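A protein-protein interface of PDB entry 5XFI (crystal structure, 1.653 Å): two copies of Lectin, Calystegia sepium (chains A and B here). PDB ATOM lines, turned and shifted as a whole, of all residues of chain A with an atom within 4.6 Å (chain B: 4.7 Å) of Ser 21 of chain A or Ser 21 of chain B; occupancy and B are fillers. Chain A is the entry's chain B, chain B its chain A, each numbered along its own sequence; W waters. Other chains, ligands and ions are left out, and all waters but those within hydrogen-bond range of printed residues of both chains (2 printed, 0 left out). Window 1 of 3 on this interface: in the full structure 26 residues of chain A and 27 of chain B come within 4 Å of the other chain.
OG of Ser 21 of chain B is in hydrogen-bond range of OH of Tyr 149 of chain B (2.7 Å).
N of Phe 22 of chain B lies within hydrogen-bond range of O of Phe 135 of chain B.
The side-chain hydroxyl (OG) of Ser 21 of chain A sits at hydrogen-bond distance from the side-chain hydroxyl (OH) of Tyr 149 of chain A, 2.6 Å away.
The backbone carbonyl oxygen of Phe 135 of chain A lies within hydrogen-bond range of the backbone NH of Phe 22 of chain A (2.7 Å).
Water W1 bridges the side-chain hydroxyl of Tyr 149 of chain B (2.7 Å) and the side-chain hydroxyl of Tyr 149 of chain A (2.7 Å).
Water W2 bridges N of Phe 19 of chain A (2.9 Å) and NH2 of Arg 23 of chain B (3.5 Å).
Of the 9 printed residues of chain A, 7 touch a printed residue of chain B.
Printed residues of chain A that touch a printed residue of chain B: Phe 19, Trp 20, Ser 21, Phe 22, Arg 23, Ile 59 and Tyr 149.
Hydrophobic or aromatic side chains of chain A that line the printed part of chain B: Phe 19, Trp 20, Ile 59 and Tyr 149.
Along chain B the printed residues that touch a printed residue of chain A span positions 19 to 149.
O of Phe 19 of chain B lies within hydrogen-bond range of NE of Arg 23 of chain A (3.1 Å).
The side-chain hydroxyl (OG) of Ser 21 of chain B lies within hydrogen-bond range of the side-chain hydroxyl (OG) of Ser 21 of chain A (2.6 Å).
The backbone carbonyl oxygen (O) of Ser 21 of chain B is in hydrogen-bond range of the backbone NH (N) of Arg 23 of chain A (2.8 Å).
The guanidinium group (NE) of Arg 23 of chain B sits close to the backbone carbonyl oxygen (O) of Phe 19 of chain A (3.1 Å).
N of Arg 23 of chain B is in hydrogen-bond range of O of Ser 21 of chain A, at 2.8 Å.
The side-chain hydroxyl (OH) of Tyr 149 of chain B sits at hydrogen-bond distance from the side-chain hydroxyl (OH) of Tyr 149 of chain A.
Among the printed residues, merely in contact across the chains: Trp 20 of chain A with Arg 23 of chain B (3.2 Å), Arg 23 of chain A with Trp 20 of chain B (3.2 Å), Phe 22 of chain A with Ser 21 of chain B (3.4 Å), Ser 21 of chain A with Phe 22 of chain B (3.5 Å), Phe 19 of chain A with Tyr 149 of chain B (3.7 Å), Ser 21 of chain A with Tyr 149 of chain B (3.7 Å), Tyr 149 of chain A with Ser 21 of chain B (3.7 Å), Tyr 149 of chain A with Phe 19 of chain B (3.7 Å), Arg 23 of chain A with Ile 59 of chain B (3.8 Å) and Ile 59 of chain A with Arg 23 of chain B (3.8 Å).
Phe 19 of chain A touches Arg 23 of chain B, and with the chains exchanged Arg 23 of chain A touches Phe 19 of chain B.
Phe 19 of chain A touches Tyr 149 of chain B, and with the chains exchanged Tyr 149 of chain A touches Phe 19 of chain B.
Ser 21 of chain A touches Tyr 149 of chain B, and with the chains exchanged Tyr 149 of chain A touches Ser 21 of chain B.
Tyr 149 of chain A touches its own counterpart, Tyr 149 of chain B.
9 positions are printed for both chains.
Of the printed residues of chain B, Trp 20 of chain A touches Arg 23.
Of chain B, only Ser 21 (2.6 Å), Phe 22 (3.5 Å), Arg 23 (2.8 Å) and Tyr 149 (3.7 Å) come within 4 Å of Ser 21 of chain A.
Printed residues of chain B within 4 Å of Phe 22 of chain A: Ser 21.
Of the printed residues of chain B, Arg 23 of chain A touches Phe 19 (3.1 Å), Trp 20 (3.2 Å), Ser 21 (2.8 Å) and Ile 59 (3.8 Å).
Phe 135 of chain A touches none of the printed residues of chain B.
Of the printed residues of chain A, Phe 19 of chain B touches Arg 23 and Tyr 149.
Of chain A, only Ser 21 (2.6 Å), Phe 22 (3.4 Å), Arg 23 (2.8 Å) and Tyr 149 (3.7 Å) come within 4 Å of Ser 21 of chain B.
Printed residues of chain A within 4 Å of Tyr 149 of chain B: Phe 19, Ser 21 and Tyr 149.
The nearest printed residue of chain A that does not touch Ser 21 of chain B is Phe 19 of chain A (6.1 Å).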
ATOM      1  N   PHE A  19     -23.135 -33.125  -2.910  1.00  0.00           N
ATOM      2  CA  PHE A  19     -22.039 -32.723  -2.033  1.00  0.00           C
ATOM      3  C   PHE A  19     -22.012 -31.209  -1.834  1.00  0.00           C
ATOM      4  O   PHE A  19     -22.295 -30.439  -2.748  1.00  0.00           O
ATOM      5  CB  PHE A  19     -20.702 -33.187  -2.632  1.00  0.00           C
ATOM      6  CG  PHE A  19     -19.487 -32.786  -1.821  1.00  0.00           C
ATOM      7  CD1 PHE A  19     -19.260 -33.332  -0.548  1.00  0.00           C
ATOM      8  CD2 PHE A  19     -18.567 -31.880  -2.345  1.00  0.00           C
ATOM      9  CE1 PHE A  19     -18.130 -32.959   0.178  1.00  0.00           C
ATOM     10  CE2 PHE A  19     -17.443 -31.498  -1.612  1.00  0.00           C
ATOM     11  CZ  PHE A  19     -17.240 -32.043  -0.338  1.00  0.00           C
ATOM     12  N   TRP A  20     -21.646 -30.777  -0.626  1.00  0.00           N
ATOM     13  CA  TRP A  20     -21.424 -29.360  -0.369  1.00  0.00           C
ATOM     14  C   TRP A  20     -20.258 -29.237   0.586  1.00  0.00           C
ATOM     15  O   TRP A  20     -19.957 -30.167   1.345  1.00  0.00           O
ATOM     16  CB  TRP A  20     -22.672 -28.662   0.205  1.00  0.00           C
ATOM     17  CG  TRP A  20     -23.223 -29.262   1.464  1.00  0.00           C
ATOM     18  CD1 TRP A  20     -24.199 -30.197   1.559  1.00  0.00           C
ATOM     19  CD2 TRP A  20     -22.845 -28.928   2.826  1.00  0.00           C
ATOM     20  NE1 TRP A  20     -24.473 -30.478   2.883  1.00  0.00           N
ATOM     21  CE2 TRP A  20     -23.640 -29.727   3.680  1.00  0.00           C
ATOM     22  CE3 TRP A  20     -21.901 -28.056   3.388  1.00  0.00           C
ATOM     23  CZ2 TRP A  20     -23.532 -29.681   5.081  1.00  0.00           C
ATOM     24  CZ3 TRP A  20     -21.792 -28.005   4.791  1.00  0.00           C
ATOM     25  CH2 TRP A  20     -22.601 -28.828   5.612  1.00  0.00           C
ATOM     26  N   SER A  21     -19.643 -28.049   0.589  1.00  0.00           N
ATOM     27  CA  SER A  21     -18.478 -27.803   1.434  1.00  0.00           C
ATOM     28  C   SER A  21     -18.319 -26.307   1.681  1.00  0.00           C
ATOM     29  O   SER A  21     -18.487 -25.490   0.765  1.00  0.00           O
ATOM     30  CB  SER A  21     -17.211 -28.375   0.779  1.00  0.00           C
ATOM     31  OG  SER A  21     -16.048 -28.144   1.595  1.00  0.00           O
ATOM     32  N   PHE A  22     -17.975 -25.953   2.924  1.00  0.00           N
ATOM     33  CA  PHE A  22     -17.794 -24.543   3.272  1.00  0.00           C
ATOM     34  C   PHE A  22     -16.760 -24.422   4.380  1.00  0.00           C
ATOM     35  O   PHE A  22     -17.065 -24.702   5.543  1.00  0.00           O
ATOM     36  CB  PHE A  22     -19.122 -23.956   3.716  1.00  0.00           C
ATOM     37  CG  PHE A  22     -19.070 -22.490   4.062  1.00  0.00           C
ATOM     38  CD1 PHE A  22     -18.912 -21.521   3.065  1.00  0.00           C
ATOM     39  CD2 PHE A  22     -19.256 -22.073   5.385  1.00  0.00           C
ATOM     40  CE1 PHE A  22     -18.922 -20.134   3.387  1.00  0.00           C
ATOM     41  CE2 PHE A  22     -19.248 -20.709   5.722  1.00  0.00           C
ATOM     42  CZ  PHE A  22     -19.068 -19.731   4.716  1.00  0.00           C
ATOM     43  N   ARG A  23     -15.576 -23.937   4.031  1.00  0.00           N
ATOM     44  CA  ARG A  23     -14.515 -23.663   5.005  1.00  0.00           C
ATOM     45  C   ARG A  23     -14.017 -22.264   4.671  1.00  0.00           C
ATOM     46  O   ARG A  23     -13.140 -22.091   3.816  1.00  0.00           O
ATOM     47  CB  ARG A  23     -13.406 -24.718   4.925  1.00  0.00           C
ATOM     48  CG  ARG A  23     -12.497 -24.831   6.158  1.00  0.00           C
ATOM     49  CD  ARG A  23     -11.742 -23.525   6.461  1.00  0.00           C
ATOM     50  NE  ARG A  23     -10.512 -23.783   7.202  1.00  0.00           N
ATOM     51  CZ  ARG A  23      -9.756 -22.854   7.773  1.00  0.00           C
ATOM     52  NH1 ARG A  23     -10.096 -21.557   7.725  1.00  0.00           N
ATOM     53  NH2 ARG A  23      -8.639 -23.234   8.393  1.00  0.00           N
ATOM     54  N   ILE A  59     -23.002 -19.808   3.172  1.00  0.00           N
ATOM     55  CA  ILE A  59     -23.547 -20.902   2.382  1.00  0.00           C
ATOM     56  C   ILE A  59     -24.857 -21.302   3.024  1.00  0.00           C
ATOM     57  O   ILE A  59     -24.985 -21.264   4.250  1.00  0.00           O
ATOM     58  CB  ILE A  59     -22.567 -22.097   2.295  1.00  0.00           C
ATOM     59  CG1 ILE A  59     -22.998 -23.039   1.174  1.00  0.00           C
ATOM     60  CG2 ILE A  59     -22.501 -22.860   3.637  1.00  0.00           C
ATOM     61  CD1 ILE A  59     -22.030 -24.166   0.914  1.00  0.00           C
ATOM     62  N   PHE A 135     -17.572 -26.787   7.435  1.00  0.00           N
ATOM     63  CA  PHE A 135     -18.459 -27.934   7.369  1.00  0.00           C
ATOM     64  C   PHE A 135     -18.507 -28.454   5.940  1.00  0.00           C
ATOM     65  O   PHE A 135     -18.179 -27.747   4.988  1.00  0.00           O
ATOM     66  CB  PHE A 135     -19.889 -27.599   7.844  1.00  0.00           C
ATOM     67  CG  PHE A 135     -19.966 -27.164   9.290  1.00  0.00           C
ATOM     68  CD1 PHE A 135     -20.180 -28.102  10.299  1.00  0.00           C
ATOM     69  CD2 PHE A 135     -19.834 -25.824   9.641  1.00  0.00           C
ATOM     70  CE1 PHE A 135     -20.253 -27.705  11.651  1.00  0.00           C
ATOM     71  CE2 PHE A 135     -19.888 -25.423  10.992  1.00  0.00           C
ATOM     72  CZ  PHE A 135     -20.099 -26.350  11.981  1.00  0.00           C
ATOM     73  N   LEU A 136     -18.917 -29.711   5.821  1.00  0.00           N
ATOM     74  CA  LEU A 136     -19.126 -30.334   4.521  1.00  0.00           C
ATOM     75  C   LEU A 136     -20.217 -31.387   4.691  1.00  0.00           C
ATOM     76  O   LEU A 136     -20.617 -31.730   5.812  1.00  0.00           O
ATOM     77  CB  LEU A 136     -17.825 -30.944   3.948  1.00  0.00           C
ATOM     78  CG  LEU A 136     -17.279 -32.249   4.572  1.00  0.00           C
ATOM     79  CD1 LEU A 136     -16.167 -32.752   3.687  1.00  0.00           C
ATOM     80  CD2 LEU A 136     -16.740 -31.972   5.964  1.00  0.00           C
ATOM     81  N   TYR A 149     -14.584 -29.714   9.097  1.00  0.00           N
ATOM     82  CA  TYR A 149     -13.167 -29.426   8.923  1.00  0.00           C
ATOM     83  C   TYR A 149     -12.620 -28.943  10.259  1.00  0.00           C
ATOM     84  O   TYR A 149     -13.286 -28.183  10.969  1.00  0.00           O
ATOM     85  CB  TYR A 149     -12.917 -28.336   7.865  1.00  0.00           C
ATOM     86  CG  TYR A 149     -13.282 -28.758   6.472  1.00  0.00           C
ATOM     87  CD1 TYR A 149     -12.460 -29.615   5.734  1.00  0.00           C
ATOM     88  CD2 TYR A 149     -14.450 -28.291   5.887  1.00  0.00           C
ATOM     89  CE1 TYR A 149     -12.828 -30.014   4.429  1.00  0.00           C
ATOM     90  CE2 TYR A 149     -14.806 -28.655   4.600  1.00  0.00           C
ATOM     91  CZ  TYR A 149     -13.997 -29.501   3.873  1.00  0.00           C
ATOM     92  OH  TYR A 149     -14.402 -29.876   2.584  1.00  0.00           O
ATOM     93  N   PHE B  19      -6.226 -23.173   4.914  1.00  0.00           N
ATOM     94  CA  PHE B  19      -7.118 -23.931   4.041  1.00  0.00           C
ATOM     95  C   PHE B  19      -8.460 -23.222   3.859  1.00  0.00           C
ATOM     96  O   PHE B  19      -8.994 -22.616   4.785  1.00  0.00           O
ATOM     97  CB  PHE B  19      -7.351 -25.330   4.632  1.00  0.00           C
ATOM     98  CG  PHE B  19      -8.301 -26.205   3.821  1.00  0.00           C
ATOM     99  CD1 PHE B  19      -7.926 -26.701   2.567  1.00  0.00           C
ATOM    100  CD2 PHE B  19      -9.551 -26.554   4.340  1.00  0.00           C
ATOM    101  CE1 PHE B  19      -8.805 -27.521   1.840  1.00  0.00           C
ATOM    102  CE2 PHE B  19     -10.436 -27.364   3.612  1.00  0.00           C
ATOM    103  CZ  PHE B  19     -10.052 -27.850   2.360  1.00  0.00           C
ATOM    104  N   TRP B  20      -9.027 -23.334   2.657  1.00  0.00           N
ATOM    105  CA  TRP B  20     -10.368 -22.830   2.398  1.00  0.00           C
ATOM    106  C   TRP B  20     -11.060 -23.790   1.451  1.00  0.00           C
ATOM    107  O   TRP B  20     -10.410 -24.513   0.677  1.00  0.00           O
ATOM    108  CB  TRP B  20     -10.360 -21.394   1.817  1.00  0.00           C
ATOM    109  CG  TRP B  20      -9.577 -21.220   0.528  1.00  0.00           C
ATOM    110  CD1 TRP B  20      -8.287 -20.802   0.414  1.00  0.00           C
ATOM    111  CD2 TRP B  20     -10.049 -21.430  -0.821  1.00  0.00           C
ATOM    112  NE1 TRP B  20      -7.918 -20.735  -0.898  1.00  0.00           N
ATOM    113  CE2 TRP B  20      -8.975 -21.125  -1.683  1.00  0.00           C
ATOM    114  CE3 TRP B  20     -11.275 -21.823  -1.375  1.00  0.00           C
ATOM    115  CZ2 TRP B  20      -9.075 -21.219  -3.084  1.00  0.00           C
ATOM    116  CZ3 TRP B  20     -11.375 -21.925  -2.759  1.00  0.00           C
ATOM    117  CH2 TRP B  20     -10.273 -21.638  -3.593  1.00  0.00           C
ATOM    118  N   SER B  21     -12.393 -23.764   1.484  1.00  0.00           N
ATOM    119  CA  SER B  21     -13.173 -24.651   0.620  1.00  0.00           C
ATOM    120  C   SER B  21     -14.555 -24.067   0.344  1.00  0.00           C
ATOM    121  O   SER B  21     -15.207 -23.531   1.252  1.00  0.00           O
ATOM    122  CB  SER B  21     -13.296 -26.039   1.272  1.00  0.00           C
ATOM    123  OG  SER B  21     -14.014 -26.945   0.430  1.00  0.00           O
ATOM    124  N   PHE B  22     -15.025 -24.232  -0.903  1.00  0.00           N
ATOM    125  CA  PHE B  22     -16.335 -23.695  -1.277  1.00  0.00           C
ATOM    126  C   PHE B  22     -16.942 -24.548  -2.377  1.00  0.00           C
ATOM    127  O   PHE B  22     -16.569 -24.410  -3.542  1.00  0.00           O
ATOM    128  CB  PHE B  22     -16.193 -22.260  -1.744  1.00  0.00           C
ATOM    129  CG  PHE B  22     -17.502 -21.588  -2.062  1.00  0.00           C
ATOM    130  CD1 PHE B  22     -18.407 -21.266  -1.049  1.00  0.00           C
ATOM    131  CD2 PHE B  22     -17.806 -21.221  -3.374  1.00  0.00           C
ATOM    132  CE1 PHE B  22     -19.614 -20.568  -1.351  1.00  0.00           C
ATOM    133  CE2 PHE B  22     -19.007 -20.567  -3.684  1.00  0.00           C
ATOM    134  CZ  PHE B  22     -19.917 -20.240  -2.669  1.00  0.00           C
ATOM    135  N   ARG B  23     -17.916 -25.372  -2.012  1.00  0.00           N
ATOM    136  CA  ARG B  23     -18.693 -26.140  -2.985  1.00  0.00           C
ATOM    137  C   ARG B  23     -20.160 -25.893  -2.655  1.00  0.00           C
ATOM    138  O   ARG B  23     -20.737 -26.580  -1.792  1.00  0.00           O
ATOM    139  CB  ARG B  23     -18.332 -27.625  -2.925  1.00  0.00           C
ATOM    140  CG  ARG B  23     -18.652 -28.420  -4.202  1.00  0.00           C
ATOM    141  CD  ARG B  23     -20.150 -28.488  -4.480  1.00  0.00           C
ATOM    142  NE  ARG B  23     -20.505 -29.681  -5.226  1.00  0.00           N
ATOM    143  CZ  ARG B  23     -21.695 -29.919  -5.753  1.00  0.00           C
ATOM    144  NH1 ARG B  23     -22.688 -29.017  -5.674  1.00  0.00           N
ATOM    145  NH2 ARG B  23     -21.890 -31.079  -6.381  1.00  0.00           N
ATOM    146  N   ILE B  59     -17.937 -16.831  -1.141  1.00  0.00           N
ATOM    147  CA  ILE B  59     -16.699 -16.898  -0.377  1.00  0.00           C
ATOM    148  C   ILE B  59     -15.700 -15.953  -1.020  1.00  0.00           C
ATOM    149  O   ILE B  59     -15.654 -15.824  -2.247  1.00  0.00           O
ATOM    150  CB  ILE B  59     -16.139 -18.343  -0.317  1.00  0.00           C
ATOM    151  CG1 ILE B  59     -15.092 -18.448   0.788  1.00  0.00           C
ATOM    152  CG2 ILE B  59     -15.522 -18.750  -1.665  1.00  0.00           C
ATOM    153  CD1 ILE B  59     -14.628 -19.884   1.090  1.00  0.00           C
ATOM    154  N   PHE B 135     -14.483 -25.007  -5.425  1.00  0.00           N
ATOM    155  CA  PHE B 135     -13.049 -24.789  -5.352  1.00  0.00           C
ATOM    156  C   PHE B 135     -12.577 -24.987  -3.918  1.00  0.00           C
ATOM    157  O   PHE B 135     -13.363 -24.951  -2.972  1.00  0.00           O
ATOM    158  CB  PHE B 135     -12.654 -23.378  -5.840  1.00  0.00           C
ATOM    159  CG  PHE B 135     -13.007 -23.098  -7.281  1.00  0.00           C
ATOM    160  CD1 PHE B 135     -12.071 -23.337  -8.296  1.00  0.00           C
ATOM    161  CD2 PHE B 135     -14.238 -22.575  -7.620  1.00  0.00           C
ATOM    162  CE1 PHE B 135     -12.374 -23.081  -9.626  1.00  0.00           C
ATOM    163  CE2 PHE B 135     -14.560 -22.323  -8.975  1.00  0.00           C
ATOM    164  CZ  PHE B 135     -13.634 -22.572  -9.954  1.00  0.00           C
ATOM    165  N   LEU B 136     -11.280 -25.244  -3.786  1.00  0.00           N
ATOM    166  CA  LEU B 136     -10.633 -25.349  -2.484  1.00  0.00           C
ATOM    167  C   LEU B 136      -9.178 -24.928  -2.653  1.00  0.00           C
ATOM    168  O   LEU B 136      -8.673 -24.764  -3.772  1.00  0.00           O
ATOM    169  CB  LEU B 136     -10.758 -26.773  -1.883  1.00  0.00           C
ATOM    170  CG  LEU B 136      -9.905 -27.892  -2.503  1.00  0.00           C
ATOM    171  CD1 LEU B 136      -9.978 -29.102  -1.614  1.00  0.00           C
ATOM    172  CD2 LEU B 136     -10.435 -28.264  -3.910  1.00  0.00           C
ATOM    173  N   TYR B 149     -13.386 -28.995  -7.079  1.00  0.00           N
ATOM    174  CA  TYR B 149     -14.326 -30.093  -6.891  1.00  0.00           C
ATOM    175  C   TYR B 149     -15.010 -30.358  -8.225  1.00  0.00           C
ATOM    176  O   TYR B 149     -15.322 -29.418  -8.963  1.00  0.00           O
ATOM    177  CB  TYR B 149     -15.401 -29.771  -5.838  1.00  0.00           C
ATOM    178  CG  TYR B 149     -14.849 -29.667  -4.446  1.00  0.00           C
ATOM    179  CD1 TYR B 149     -14.492 -30.801  -3.722  1.00  0.00           C
ATOM    180  CD2 TYR B 149     -14.714 -28.428  -3.840  1.00  0.00           C
ATOM    181  CE1 TYR B 149     -13.977 -30.688  -2.429  1.00  0.00           C
ATOM    182  CE2 TYR B 149     -14.208 -28.309  -2.556  1.00  0.00           C
ATOM    183  CZ  TYR B 149     -13.863 -29.440  -1.855  1.00  0.00           C
ATOM    184  OH  TYR B 149     -13.342 -29.316  -0.564  1.00  0.00           O
HETATM  185  O   HOH W   1     -12.797 -31.464   1.023  1.00  0.00           O
HETATM  186  O   HOH W   2     -22.286 -34.395  -5.397  1.00  0.00           O
